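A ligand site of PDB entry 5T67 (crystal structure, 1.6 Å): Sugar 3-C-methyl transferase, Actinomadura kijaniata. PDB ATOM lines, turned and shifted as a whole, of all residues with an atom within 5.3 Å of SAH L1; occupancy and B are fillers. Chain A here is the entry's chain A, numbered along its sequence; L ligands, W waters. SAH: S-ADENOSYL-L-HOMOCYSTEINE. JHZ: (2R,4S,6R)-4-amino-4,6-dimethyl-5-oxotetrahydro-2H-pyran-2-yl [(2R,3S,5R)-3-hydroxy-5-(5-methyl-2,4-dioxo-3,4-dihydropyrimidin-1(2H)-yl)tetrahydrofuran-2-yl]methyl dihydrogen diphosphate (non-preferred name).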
ATOM      1  N   ARG A  70      24.061  -0.449 -31.994  1.00  0.00           N
ATOM      2  CA  ARG A  70      23.716   0.887 -31.464  1.00  0.00           C
ATOM      3  C   ARG A  70      22.996   0.934 -30.126  1.00  0.00           C
ATOM      4  O   ARG A  70      23.219   1.871 -29.358  1.00  0.00           O
ATOM      5  CB  ARG A  70      22.920   1.681 -32.531  1.00  0.00           C
ATOM      6  CG  ARG A  70      21.502   1.224 -32.726  1.00  0.00           C
ATOM      7  CD  ARG A  70      20.778   1.963 -33.820  1.00  0.00           C
ATOM      8  NE  ARG A  70      19.428   1.465 -33.993  1.00  0.00           N
ATOM      9  CZ  ARG A  70      18.607   1.946 -34.921  1.00  0.00           C
ATOM     10  NH1 ARG A  70      18.984   2.961 -35.713  1.00  0.00           N
ATOM     11  NH2 ARG A  70      17.360   1.430 -35.028  1.00  0.00           N
ATOM     12  N   PHE A  74      23.718   3.523 -27.040  1.00  0.00           N
ATOM     13  CA  PHE A  74      22.791   4.606 -26.867  1.00  0.00           C
ATOM     14  C   PHE A  74      21.439   4.067 -26.379  1.00  0.00           C
ATOM     15  O   PHE A  74      20.849   3.261 -27.078  1.00  0.00           O
ATOM     16  CB  PHE A  74      22.618   5.319 -28.164  1.00  0.00           C
ATOM     17  CG  PHE A  74      23.936   5.666 -28.824  1.00  0.00           C
ATOM     18  CD1 PHE A  74      24.809   6.573 -28.203  1.00  0.00           C
ATOM     19  CD2 PHE A  74      24.332   5.101 -30.039  1.00  0.00           C
ATOM     20  CE1 PHE A  74      26.052   6.916 -28.786  1.00  0.00           C
ATOM     21  CE2 PHE A  74      25.578   5.429 -30.613  1.00  0.00           C
ATOM     22  CZ  PHE A  74      26.428   6.347 -30.011  1.00  0.00           C
ATOM     23  N   TYR A  78      22.528   6.405 -21.056  1.00  0.00           N
ATOM     24  CA  TYR A  78      23.714   7.012 -21.694  1.00  0.00           C
ATOM     25  C   TYR A  78      24.174   8.207 -20.822  1.00  0.00           C
ATOM     26  O   TYR A  78      23.339   9.074 -20.564  1.00  0.00           O
ATOM     27  CB  TYR A  78      23.340   7.489 -23.084  1.00  0.00           C
ATOM     28  CG  TYR A  78      24.513   8.069 -23.850  1.00  0.00           C
ATOM     29  CD1 TYR A  78      24.580   9.434 -24.098  1.00  0.00           C
ATOM     30  CD2 TYR A  78      25.570   7.314 -24.280  1.00  0.00           C
ATOM     31  CE1 TYR A  78      25.594   9.973 -24.860  1.00  0.00           C
ATOM     32  CE2 TYR A  78      26.611   7.845 -25.031  1.00  0.00           C
ATOM     33  CZ  TYR A  78      26.641   9.211 -25.297  1.00  0.00           C
ATOM     34  OH  TYR A  78      27.690   9.665 -25.985  1.00  0.00           O
ATOM     35  N   TYR A  80      26.719  10.690 -21.034  1.00  0.00           N
ATOM     36  CA  TYR A  80      27.309  11.996 -21.439  1.00  0.00           C
ATOM     37  C   TYR A  80      26.216  13.070 -21.530  1.00  0.00           C
ATOM     38  O   TYR A  80      25.370  12.984 -22.423  1.00  0.00           O
ATOM     39  CB  TYR A  80      28.034  11.835 -22.762  1.00  0.00           C
ATOM     40  CG  TYR A  80      28.808  13.114 -23.144  1.00  0.00           C
ATOM     41  CD1 TYR A  80      29.974  13.497 -22.474  1.00  0.00           C
ATOM     42  CD2 TYR A  80      28.346  13.985 -24.124  1.00  0.00           C
ATOM     43  CE1 TYR A  80      30.626  14.686 -22.700  1.00  0.00           C
ATOM     44  CE2 TYR A  80      29.047  15.196 -24.400  1.00  0.00           C
ATOM     45  CZ  TYR A  80      30.223  15.509 -23.722  1.00  0.00           C
ATOM     46  OH  TYR A  80      30.931  16.648 -24.072  1.00  0.00           O
ATOM     47  N   SER A  82      25.936  16.875 -22.515  1.00  0.00           N
ATOM     48  CA  SER A  82      26.698  17.873 -23.279  1.00  0.00           C
ATOM     49  C   SER A  82      26.857  19.187 -22.517  1.00  0.00           C
ATOM     50  O   SER A  82      27.860  19.846 -22.645  1.00  0.00           O
ATOM     51  CB  SER A  82      25.890  18.190 -24.508  1.00  0.00           C
ATOM     52  OG  SER A  82      25.763  17.087 -25.334  1.00  0.00           O
ATOM     53  N   PHE A  92      27.455  25.994 -28.636  1.00  0.00           N
ATOM     54  CA  PHE A  92      26.170  25.664 -29.188  1.00  0.00           C
ATOM     55  C   PHE A  92      25.170  26.831 -29.221  1.00  0.00           C
ATOM     56  O   PHE A  92      24.358  26.892 -30.147  1.00  0.00           O
ATOM     57  CB  PHE A  92      25.623  24.381 -28.563  1.00  0.00           C
ATOM     58  CG  PHE A  92      26.359  23.165 -29.034  1.00  0.00           C
ATOM     59  CD1 PHE A  92      26.381  22.806 -30.390  1.00  0.00           C
ATOM     60  CD2 PHE A  92      27.119  22.430 -28.115  1.00  0.00           C
ATOM     61  CE1 PHE A  92      27.097  21.713 -30.802  1.00  0.00           C
ATOM     62  CE2 PHE A  92      27.829  21.307 -28.504  1.00  0.00           C
ATOM     63  CZ  PHE A  92      27.825  20.991 -29.850  1.00  0.00           C
ATOM     64  N   GLU A 113      17.457  18.641 -35.232  1.00  0.00           N
ATOM     65  CA  GLU A 113      18.788  18.156 -34.760  1.00  0.00           C
ATOM     66  C   GLU A 113      18.797  16.655 -34.526  1.00  0.00           C
ATOM     67  O   GLU A 113      17.926  16.105 -33.825  1.00  0.00           O
ATOM     68  CB  GLU A 113      19.171  18.818 -33.469  1.00  0.00           C
ATOM     69  CG  GLU A 113      20.613  18.458 -33.070  1.00  0.00           C
ATOM     70  CD  GLU A 113      21.174  19.296 -31.931  1.00  0.00           C
ATOM     71  OE1 GLU A 113      22.422  19.255 -31.706  1.00  0.00           O
ATOM     72  OE2 GLU A 113      20.434  19.987 -31.221  1.00  0.00           O
ATOM     73  N   ILE A 114      19.864  15.997 -34.992  1.00  0.00           N
ATOM     74  CA  ILE A 114      20.092  14.610 -34.691  1.00  0.00           C
ATOM     75  C   ILE A 114      21.113  14.558 -33.549  1.00  0.00           C
ATOM     76  O   ILE A 114      22.187  15.145 -33.686  1.00  0.00           O
ATOM     77  CB  ILE A 114      20.746  13.956 -35.922  1.00  0.00           C
ATOM     78  CG1 ILE A 114      19.858  14.080 -37.175  1.00  0.00           C
ATOM     79  CG2 ILE A 114      21.131  12.524 -35.684  1.00  0.00           C
ATOM     80  CD1 ILE A 114      20.544  13.522 -38.387  1.00  0.00           C
ATOM     81  N   GLY A 115      20.799  13.904 -32.442  1.00  0.00           N
ATOM     82  CA  GLY A 115      21.702  13.754 -31.304  1.00  0.00           C
ATOM     83  C   GLY A 115      21.687  15.035 -30.462  1.00  0.00           C
ATOM     84  O   GLY A 115      22.719  15.489 -29.994  1.00  0.00           O
ATOM     85  N   CYS A 116      20.487  15.532 -30.149  1.00  0.00           N
ATOM     86  CA  CYS A 116      20.398  16.791 -29.393  1.00  0.00           C
ATOM     87  C   CYS A 116      20.740  16.653 -27.947  1.00  0.00           C
ATOM     88  O   CYS A 116      20.995  17.658 -27.294  1.00  0.00           O
ATOM     89  CB  CYS A 116      19.020  17.512 -29.479  1.00  0.00           C
ATOM     90  SG  CYS A 116      17.692  16.499 -28.816  1.00  0.00           S
ATOM     91  N   ASN A 117      20.837  15.438 -27.408  1.00  0.00           N
ATOM     92  CA  ASN A 117      21.324  15.223 -26.051  1.00  0.00           C
ATOM     93  C   ASN A 117      20.399  16.019 -25.101  1.00  0.00           C
ATOM     94  O   ASN A 117      19.128  16.030 -25.289  1.00  0.00           O
ATOM     95  CB  ASN A 117      22.841  15.473 -25.981  1.00  0.00           C
ATOM     96  CG  ASN A 117      23.517  14.932 -24.729  1.00  0.00           C
ATOM     97  OD1 ASN A 117      23.593  15.597 -23.674  1.00  0.00           O
ATOM     98  ND2 ASN A 117      24.037  13.737 -24.828  1.00  0.00           N
ATOM     99  N   ILE A 120      21.462  21.334 -25.496  1.00  0.00           N
ATOM    100  CA  ILE A 120      22.515  22.361 -25.475  1.00  0.00           C
ATOM    101  C   ILE A 120      22.389  23.297 -26.665  1.00  0.00           C
ATOM    102  O   ILE A 120      22.624  24.465 -26.466  1.00  0.00           O
ATOM    103  CB  ILE A 120      23.926  21.685 -25.407  1.00  0.00           C
ATOM    104  CG1 ILE A 120      25.035  22.669 -25.018  1.00  0.00           C
ATOM    105  CG2 ILE A 120      24.186  20.884 -26.683  1.00  0.00           C
ATOM    106  CD1 ILE A 120      26.307  21.980 -24.551  1.00  0.00           C
ATOM    107  N   PHE A 135      16.018  14.499 -32.439  1.00  0.00           N
ATOM    108  CA  PHE A 135      15.959  13.020 -32.356  1.00  0.00           C
ATOM    109  C   PHE A 135      17.046  12.658 -31.338  1.00  0.00           C
ATOM    110  O   PHE A 135      18.242  12.969 -31.598  1.00  0.00           O
ATOM    111  CB  PHE A 135      16.303  12.371 -33.675  1.00  0.00           C
ATOM    112  CG  PHE A 135      15.217  12.491 -34.738  1.00  0.00           C
ATOM    113  CD1 PHE A 135      14.503  11.403 -35.163  1.00  0.00           C
ATOM    114  CD2 PHE A 135      15.049  13.677 -35.375  1.00  0.00           C
ATOM    115  CE1 PHE A 135      13.513  11.552 -36.138  1.00  0.00           C
ATOM    116  CE2 PHE A 135      14.095  13.831 -36.411  1.00  0.00           C
ATOM    117  CZ  PHE A 135      13.311  12.750 -36.765  1.00  0.00           C
ATOM    118  N   GLU A 136      16.661  12.018 -30.238  1.00  0.00           N
ATOM    119  CA  GLU A 136      17.597  11.612 -29.178  1.00  0.00           C
ATOM    120  C   GLU A 136      17.154  10.259 -28.614  1.00  0.00           C
ATOM    121  O   GLU A 136      16.252  10.258 -27.786  1.00  0.00           O
ATOM    122  CB  GLU A 136      17.618  12.726 -28.126  1.00  0.00           C
ATOM    123  CG  GLU A 136      18.647  12.538 -26.996  1.00  0.00           C
ATOM    124  CD  GLU A 136      19.926  11.903 -27.561  1.00  0.00           C
ATOM    125  OE1 GLU A 136      20.783  12.682 -28.022  1.00  0.00           O
ATOM    126  OE2 GLU A 136      20.025  10.639 -27.549  1.00  0.00           O
ATOM    127  N   PRO A 137      17.732   9.144 -29.087  1.00  0.00           N
ATOM    128  CA  PRO A 137      17.306   7.842 -28.614  1.00  0.00           C
ATOM    129  C   PRO A 137      17.759   7.498 -27.241  1.00  0.00           C
ATOM    130  O   PRO A 137      17.319   6.463 -26.757  1.00  0.00           O
ATOM    131  CB  PRO A 137      17.942   6.898 -29.593  1.00  0.00           C
ATOM    132  CG  PRO A 137      19.235   7.584 -29.987  1.00  0.00           C
ATOM    133  CD  PRO A 137      18.885   9.034 -29.987  1.00  0.00           C
ATOM    134  N   SER A 138      18.576   8.337 -26.585  1.00  0.00           N
ATOM    135  CA  SER A 138      18.941   8.179 -25.213  1.00  0.00           C
ATOM    136  C   SER A 138      18.039   8.957 -24.281  1.00  0.00           C
ATOM    137  O   SER A 138      18.135  10.179 -24.110  1.00  0.00           O
ATOM    138  CB  SER A 138      20.418   8.500 -24.903  1.00  0.00           C
ATOM    139  OG  SER A 138      21.282   7.685 -25.681  1.00  0.00           O
ATOM    140  N   VAL A 141      19.087  11.832 -21.211  1.00  0.00           N
ATOM    141  CA  VAL A 141      19.511  13.183 -21.671  1.00  0.00           C
ATOM    142  C   VAL A 141      18.349  13.837 -22.391  1.00  0.00           C
ATOM    143  O   VAL A 141      18.221  15.035 -22.322  1.00  0.00           O
ATOM    144  CB  VAL A 141      20.788  13.210 -22.497  1.00  0.00           C
ATOM    145  CG1 VAL A 141      21.956  12.872 -21.582  1.00  0.00           C
ATOM    146  CG2 VAL A 141      20.739  12.151 -23.604  1.00  0.00           C
ATOM    147  N   GLU A 155      14.071   8.466 -30.381  1.00  0.00           N
ATOM    148  CA  GLU A 155      14.169   7.517 -31.468  1.00  0.00           C
ATOM    149  C   GLU A 155      15.426   7.824 -32.259  1.00  0.00           C
ATOM    150  O   GLU A 155      15.949   8.952 -32.255  1.00  0.00           O
ATOM    151  CB  GLU A 155      12.877   7.495 -32.313  1.00  0.00           C
ATOM    152  CG  GLU A 155      12.672   8.577 -33.306  1.00  0.00           C
ATOM    153  CD  GLU A 155      11.311   8.564 -34.022  1.00  0.00           C
ATOM    154  OE1 GLU A 155      11.189   9.484 -34.838  1.00  0.00           O
ATOM    155  OE2 GLU A 155      10.390   7.757 -33.817  1.00  0.00           O
ATOM    156  N   PHE A 156      15.899   6.823 -32.977  1.00  0.00           N
ATOM    157  CA  PHE A 156      17.088   6.970 -33.800  1.00  0.00           C
ATOM    158  C   PHE A 156      16.648   7.650 -35.096  1.00  0.00           C
ATOM    159  O   PHE A 156      15.653   7.242 -35.681  1.00  0.00           O
ATOM    160  CB  PHE A 156      17.740   5.638 -34.115  1.00  0.00           C
ATOM    161  CG  PHE A 156      18.383   4.958 -32.940  1.00  0.00           C
ATOM    162  CD1 PHE A 156      19.699   5.228 -32.595  1.00  0.00           C
ATOM    163  CD2 PHE A 156      17.692   4.004 -32.210  1.00  0.00           C
ATOM    164  CE1 PHE A 156      20.295   4.602 -31.518  1.00  0.00           C
ATOM    165  CE2 PHE A 156      18.232   3.417 -31.069  1.00  0.00           C
ATOM    166  CZ  PHE A 156      19.549   3.688 -30.758  1.00  0.00           C
ATOM    167  N   PHE A 157      17.383   8.644 -35.565  1.00  0.00           N
ATOM    168  CA  PHE A 157      17.210   9.214 -36.914  1.00  0.00           C
ATOM    169  C   PHE A 157      17.760   8.199 -37.897  1.00  0.00           C
ATOM    170  O   PHE A 157      18.909   7.728 -37.747  1.00  0.00           O
ATOM    171  CB  PHE A 157      18.004  10.527 -37.038  1.00  0.00           C
ATOM    172  CG  PHE A 157      17.762  11.247 -38.355  1.00  0.00           C
ATOM    173  CD1 PHE A 157      18.445  10.872 -39.506  1.00  0.00           C
ATOM    174  CD2 PHE A 157      16.841  12.279 -38.434  1.00  0.00           C
ATOM    175  CE1 PHE A 157      18.196  11.530 -40.706  1.00  0.00           C
ATOM    176  CE2 PHE A 157      16.607  12.931 -39.651  1.00  0.00           C
ATOM    177  CZ  PHE A 157      17.309  12.542 -40.775  1.00  0.00           C
ATOM    178  N   GLU A 158      16.915   7.863 -38.870  1.00  0.00           N
ATOM    179  CA  GLU A 158      17.224   6.979 -39.964  1.00  0.00           C
ATOM    180  C   GLU A 158      16.111   7.191 -41.002  1.00  0.00           C
ATOM    181  O   GLU A 158      15.172   7.933 -40.771  1.00  0.00           O
ATOM    182  CB  GLU A 158      17.186   5.503 -39.505  1.00  0.00           C
ATOM    183  CG  GLU A 158      15.910   5.125 -38.777  1.00  0.00           C
ATOM    184  CD  GLU A 158      16.006   3.708 -38.215  1.00  0.00           C
ATOM    185  OE1 GLU A 158      15.430   2.804 -38.855  1.00  0.00           O
ATOM    186  OE2 GLU A 158      16.648   3.410 -37.207  1.00  0.00           O
ATOM    187  N   ALA A 178      25.893  17.399 -34.223  1.00  0.00           N
ATOM    188  CA  ALA A 178      27.224  17.598 -33.686  1.00  0.00           C
ATOM    189  C   ALA A 178      27.627  16.353 -32.896  1.00  0.00           C
ATOM    190  O   ALA A 178      26.873  15.912 -32.041  1.00  0.00           O
ATOM    191  CB  ALA A 178      27.231  18.794 -32.766  1.00  0.00           C
ATOM    192  N   ASN A 179      28.841  15.848 -33.194  1.00  0.00           N
ATOM    193  CA  ASN A 179      29.396  14.689 -32.502  1.00  0.00           C
ATOM    194  C   ASN A 179      28.369  13.545 -32.509  1.00  0.00           C
ATOM    195  O   ASN A 179      28.166  12.893 -31.487  1.00  0.00           O
ATOM    196  CB  ASN A 179      29.787  15.124 -31.089  1.00  0.00           C
ATOM    197  CG  ASN A 179      30.646  16.370 -31.144  1.00  0.00           C
ATOM    198  OD1 ASN A 179      31.749  16.284 -31.696  1.00  0.00           O
ATOM    199  ND2 ASN A 179      30.223  17.475 -30.532  1.00  0.00           N
ATOM    200  N   THR A 180      27.677  13.435 -33.644  1.00  0.00           N
ATOM    201  CA  THR A 180      26.646  12.411 -33.836  1.00  0.00           C
ATOM    202  C   THR A 180      26.826  11.718 -35.166  1.00  0.00           C
ATOM    203  O   THR A 180      26.760  10.449 -35.221  1.00  0.00           O
ATOM    204  CB  THR A 180      25.239  13.010 -33.627  1.00  0.00           C
ATOM    205  OG1 THR A 180      25.159  13.682 -32.370  1.00  0.00           O
ATOM    206  CG2 THR A 180      24.185  11.974 -33.742  1.00  0.00           C
ATOM    207  N   HIS A 183      29.113   8.860 -35.238  1.00  0.00           N
ATOM    208  CA  HIS A 183      28.684   7.780 -34.362  1.00  0.00           C
ATOM    209  C   HIS A 183      27.758   6.822 -35.057  1.00  0.00           C
ATOM    210  O   HIS A 183      27.395   5.787 -34.457  1.00  0.00           O
ATOM    211  CB  HIS A 183      27.905   8.329 -33.173  1.00  0.00           C
ATOM    212  CG  HIS A 183      28.706   9.189 -32.234  1.00  0.00           C
ATOM    213  ND1 HIS A 183      29.601  10.150 -32.682  1.00  0.00           N
ATOM    214  CD2 HIS A 183      28.669   9.296 -30.886  1.00  0.00           C
ATOM    215  CE1 HIS A 183      30.132  10.750 -31.647  1.00  0.00           C
ATOM    216  NE2 HIS A 183      29.542  10.307 -30.556  1.00  0.00           N
ATOM    217  N   ILE A 184      27.367   7.166 -36.275  1.00  0.00           N
ATOM    218  CA  ILE A 184      26.326   6.468 -37.020  1.00  0.00           C
ATOM    219  C   ILE A 184      26.892   5.701 -38.256  1.00  0.00           C
ATOM    220  O   ILE A 184      27.153   6.289 -39.304  1.00  0.00           O
ATOM    221  CB  ILE A 184      25.178   7.412 -37.414  1.00  0.00           C
ATOM    222  CG1 ILE A 184      24.404   7.965 -36.210  1.00  0.00           C
ATOM    223  CG2 ILE A 184      24.169   6.715 -38.326  1.00  0.00           C
ATOM    224  CD1 ILE A 184      23.554   9.198 -36.461  1.00  0.00           C
ATOM    225  N   TYR A 186      25.407   3.786 -40.329  1.00  0.00           N
ATOM    226  CA  TYR A 186      24.373   3.673 -41.363  1.00  0.00           C
ATOM    227  C   TYR A 186      24.084   4.982 -42.081  1.00  0.00           C
ATOM    228  O   TYR A 186      22.944   5.477 -42.151  1.00  0.00           O
ATOM    229  CB  TYR A 186      23.130   2.946 -40.785  1.00  0.00           C
ATOM    230  CG  TYR A 186      22.655   3.472 -39.425  1.00  0.00           C
ATOM    231  CD1 TYR A 186      23.169   2.953 -38.254  1.00  0.00           C
ATOM    232  CD2 TYR A 186      21.652   4.405 -39.342  1.00  0.00           C
ATOM    233  CE1 TYR A 186      22.752   3.405 -37.013  1.00  0.00           C
ATOM    234  CE2 TYR A 186      21.252   4.868 -38.078  1.00  0.00           C
ATOM    235  CZ  TYR A 186      21.809   4.385 -36.934  1.00  0.00           C
ATOM    236  OH  TYR A 186      21.378   4.877 -35.711  1.00  0.00           O
ATOM    237  N   HIS A 256      36.632  19.887 -28.912  1.00  0.00           N
ATOM    238  CA  HIS A 256      36.833  18.470 -28.849  1.00  0.00           C
ATOM    239  C   HIS A 256      38.122  17.982 -29.528  1.00  0.00           C
ATOM    240  O   HIS A 256      38.150  16.962 -30.234  1.00  0.00           O
ATOM    241  CB  HIS A 256      35.630  17.833 -29.448  1.00  0.00           C
ATOM    242  CG  HIS A 256      34.425  17.836 -28.556  1.00  0.00           C
ATOM    243  ND1 HIS A 256      34.411  17.247 -27.313  1.00  0.00           N
ATOM    244  CD2 HIS A 256      33.194  18.380 -28.725  1.00  0.00           C
ATOM    245  CE1 HIS A 256      33.258  17.477 -26.722  1.00  0.00           C
ATOM    246  NE2 HIS A 256      32.495  18.145 -27.569  1.00  0.00           N
HETATM  247  N   SAH L   1      25.169  16.914 -30.023  1.00  0.00           N
HETATM  248  CA  SAH L   1      25.669  16.674 -28.632  1.00  0.00           C
HETATM  249  CB  SAH L   1      25.602  15.204 -28.208  1.00  0.00           C
HETATM  250  CG  SAH L   1      26.651  14.243 -28.688  1.00  0.00           C
HETATM  251  SD  SAH L   1      26.365  12.624 -27.930  1.00  0.00           S
HETATM  252  C   SAH L   1      27.082  17.227 -28.493  1.00  0.00           C
HETATM  253  O   SAH L   1      27.694  17.544 -29.507  1.00  0.00           O
HETATM  254  OXT SAH L   1      27.569  17.333 -27.377  1.00  0.00           O
HETATM  255  C5' SAH L   1      25.904  11.687 -29.346  1.00  0.00           C
HETATM  256  C4' SAH L   1      24.341  11.577 -29.306  1.00  0.00           C
HETATM  257  O4' SAH L   1      23.855  10.927 -30.494  1.00  0.00           O
HETATM  258  C3' SAH L   1      23.806  10.761 -28.099  1.00  0.00           C
HETATM  259  O3' SAH L   1      23.043  11.451 -27.103  1.00  0.00           O
HETATM  260  C2' SAH L   1      23.085   9.590 -28.711  1.00  0.00           C
HETATM  261  O2' SAH L   1      21.974   8.972 -28.074  1.00  0.00           O
HETATM  262  C1' SAH L   1      22.687  10.211 -30.072  1.00  0.00           C
HETATM  263  N9  SAH L   1      22.457   9.306 -31.198  1.00  0.00           N
HETATM  264  C8  SAH L   1      23.119   8.180 -31.554  1.00  0.00           C
HETATM  265  N7  SAH L   1      22.624   7.726 -32.714  1.00  0.00           N
HETATM  266  C5  SAH L   1      21.627   8.505 -33.105  1.00  0.00           C
HETATM  267  C6  SAH L   1      20.679   8.552 -34.237  1.00  0.00           C
HETATM  268  N6  SAH L   1      20.688   7.574 -35.202  1.00  0.00           N
HETATM  269  N1  SAH L   1      19.852   9.562 -34.174  1.00  0.00           N
HETATM  270  C2  SAH L   1      19.815  10.563 -33.261  1.00  0.00           C
HETATM  271  N3  SAH L   1      20.617  10.524 -32.208  1.00  0.00           N
HETATM  272  C4  SAH L   1      21.524   9.575 -32.113  1.00  0.00           C
HETATM  273  P   JHZ L   2      34.356  15.465 -22.931  1.00  0.00           P
HETATM  274  C1  JHZ L   2      31.812  12.366 -25.219  1.00  0.00           C
HETATM  275  O1  JHZ L   2      33.261  12.396 -25.312  1.00  0.00           O
HETATM  276  C2  JHZ L   2      31.171  11.211 -25.880  1.00  0.00           C
HETATM  277  P2  JHZ L   2      34.127  12.669 -23.958  1.00  0.00           P
HETATM  278  C3  JHZ L   2      30.824  11.555 -27.328  1.00  0.00           C
HETATM  279  N3  JHZ L   2      30.837  10.291 -28.064  1.00  0.00           N
HETATM  280  C4  JHZ L   2      31.716  12.570 -27.957  1.00  0.00           C
HETATM  281  O4  JHZ L   2      31.990  12.363 -29.130  1.00  0.00           O
HETATM  282  C5  JHZ L   2      32.115  13.818 -27.146  1.00  0.00           C
HETATM  283  O5  JHZ L   2      31.468  13.600 -25.881  1.00  0.00           O
HETATM  284  C6  JHZ L   2      31.221  14.908 -27.765  1.00  0.00           C
HETATM  285  C1X JHZ L   2      34.470  15.991 -17.115  1.00  0.00           C
HETATM  286  N11 JHZ L   2      34.922  17.340 -16.706  1.00  0.00           N
HETATM  287  O1P JHZ L   2      33.367  16.570 -23.124  1.00  0.00           O
HETATM  288  C2X JHZ L   2      33.051  16.044 -17.692  1.00  0.00           C
HETATM  289  C21 JHZ L   2      35.255  17.553 -15.428  1.00  0.00           C
HETATM  290  O21 JHZ L   2      35.279  16.623 -14.512  1.00  0.00           O
HETATM  291  O2P JHZ L   2      35.795  15.710 -23.265  1.00  0.00           O
HETATM  292  C3X JHZ L   2      33.048  14.908 -18.662  1.00  0.00           C
HETATM  293  O3X JHZ L   2      32.632  13.716 -17.959  1.00  0.00           O
HETATM  294  N31 JHZ L   2      35.692  18.736 -14.935  1.00  0.00           N
HETATM  295  C3M JHZ L   2      29.391  11.956 -27.518  1.00  0.00           C
HETATM  296  O3P JHZ L   2      35.572  12.450 -24.260  1.00  0.00           O
HETATM  297  C4X JHZ L   2      34.517  14.853 -19.100  1.00  0.00           C
HETATM  298  O4X JHZ L   2      35.313  15.592 -18.152  1.00  0.00           O
HETATM  299  C41 JHZ L   2      35.691  19.730 -15.833  1.00  0.00           C
HETATM  300  O41 JHZ L   2      36.099  20.919 -15.375  1.00  0.00           O
HETATM  301  O4P JHZ L   2      33.490  11.946 -22.876  1.00  0.00           O
HETATM  302  C5X JHZ L   2      34.776  15.662 -20.349  1.00  0.00           C
HETATM  303  O5X JHZ L   2      34.225  14.924 -21.409  1.00  0.00           O
HETATM  304  C51 JHZ L   2      35.349  19.585 -17.177  1.00  0.00           C
HETATM  305  C5A JHZ L   2      35.438  20.735 -18.159  1.00  0.00           C
HETATM  306  C61 JHZ L   2      34.938  18.345 -17.581  1.00  0.00           C
HETATM  307  OPP JHZ L   2      33.819  14.222 -23.784  1.00  0.00           O
HETATM  308  O   HOH W   1      29.843  18.674 -26.850  1.00  0.00           O
HETATM  309  O   HOH W   2      23.800  17.035 -32.474  1.00  0.00           O
HETATM  310  O   HOH W   3      23.055   4.933 -33.714  1.00  0.00           O
HETATM  311  O   HOH W   4      24.375  19.620 -30.040  1.00  0.00           O
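The side-chain amide nitrogen (ND2) of Asn 117 sits at hydrogen-bond distance from an oxygen (O3') of SAH L1, 3.4 Å away.
N of Gly 115 is in hydrogen-bond range of N3 of SAH L1 (3.4 Å).
ND2 of Asn 179 sits at hydrogen-bond distance from O of SAH L1 (2.7 Å).
N6 of SAH L1 lies within hydrogen-bond range of O of Phe 157, at 3.1 Å.
The backbone NH of Phe 157 lies within hydrogen-bond range of a nitrogen (N1) of SAH L1 (3.0 Å).
OG of Ser 82 is in hydrogen-bond range of OXT of SAH L1.
N3 of JHZ L2 sits at hydrogen-bond distance from NE2 of His 183 (2.8 Å).
SD of SAH L1 sits close to OH of Tyr 78, at 3.8 Å.
O of Gly 115 sits at hydrogen-bond distance from N of SAH L1 (2.8 Å).
The side-chain hydroxyl (OH) of Tyr 186 is in hydrogen-bond range of a nitrogen (N6) of SAH L1 (2.8 Å).
The backbone carbonyl oxygen of Ala 178 lies within hydrogen-bond range of a nitrogen (N) of SAH L1 (2.8 Å).
The side-chain carboxylate (OE1) of Glu 113 lies within salt-bridge range of a nitrogen (N) of SAH L1, at 3.98 Å.
The side-chain hydroxyl of Ser 138 lies within hydrogen-bond range of an oxygen (O2') of SAH L1, at 2.8 Å.
OH of Tyr 80 is in hydrogen-bond range of O1P of JHZ L2 (2.6 Å).
An oxygen (O2') of SAH L1 is in hydrogen-bond range of the side-chain carboxylate (OE2) of Glu 136 (2.6 Å).
A nitrogen (N3) of SAH L1 sits close to the backbone carbonyl oxygen of Phe 135 (3.5 Å).
Residues that only touch SAH L1: Phe 74 (3.5 Å), Tyr 80 (3.95 Å), Phe 92 (3.5 Å), Ile 114 (3.4 Å), Pro 137 (3.2 Å), Phe 156 (3.6 Å), Thr 180 (3.4 Å), His 183 (3.97 Å) and Ile 184 (3.5 Å).
Hydrophobic or aromatic side chains within 4 Å of SAH L1: Phe 74, Tyr 78, Tyr 80, Phe 92, Ile 114, Phe 135, Pro 137, Phe 156, Phe 157, Ala 178, His 183, Ile 184 and Tyr 186.
21 residues have an atom within 4 Å of SAH L1: Phe 74, Tyr 78, Tyr 80, Ser 82, Phe 92, Glu 113, Ile 114, Gly 115, Asn 117, Phe 135, Glu 136, Pro 137, Ser 138, Phe 156, Phe 157, Ala 178, Asn 179, Thr 180, His 183, Ile 184 and Tyr 186.
The side-chain amide nitrogen (ND2) of Asn 117 lies within hydrogen-bond range of the backbone carbonyl oxygen (O) of Tyr 80 (2.9 Å).
The backbone carbonyl oxygen (O) of Ala 178 sits at hydrogen-bond distance from the side-chain hydroxyl (OG1) of Thr 180 (2.8 Å).
N of Asn 117 is in hydrogen-bond range of OE1 of Glu 136, at 2.8 Å.
N of Gly 115 lies within hydrogen-bond range of O of Phe 135 (2.9 Å).
OE2 of Glu 136 lies within hydrogen-bond range of N of Ser 138, 2.9 Å away.
The backbone NH (N) of Phe 135 sits at hydrogen-bond distance from the backbone carbonyl oxygen (O) of Glu 113.
The side-chain hydroxyl of Tyr 186 lies within hydrogen-bond range of the guanidinium group of Arg 70 (3.1 Å).
A ring nitrogen (NE2) of His 183 lies close to the backbone carbonyl oxygen (O) of Asn 179, 3.1 Å away.
Water W1 lies within hydrogen-bond range of OXT of SAH L1 (2.7 Å) and NE2 of His 256 (2.8 Å).
Water W4 lies within hydrogen-bond range of OE1 of Glu 113 (2.6 Å) and N of SAH L1 (2.8 Å).
Water W3 bridges OH of Tyr 186 (2.6 Å) and N7 of SAH L1 (3.0 Å).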
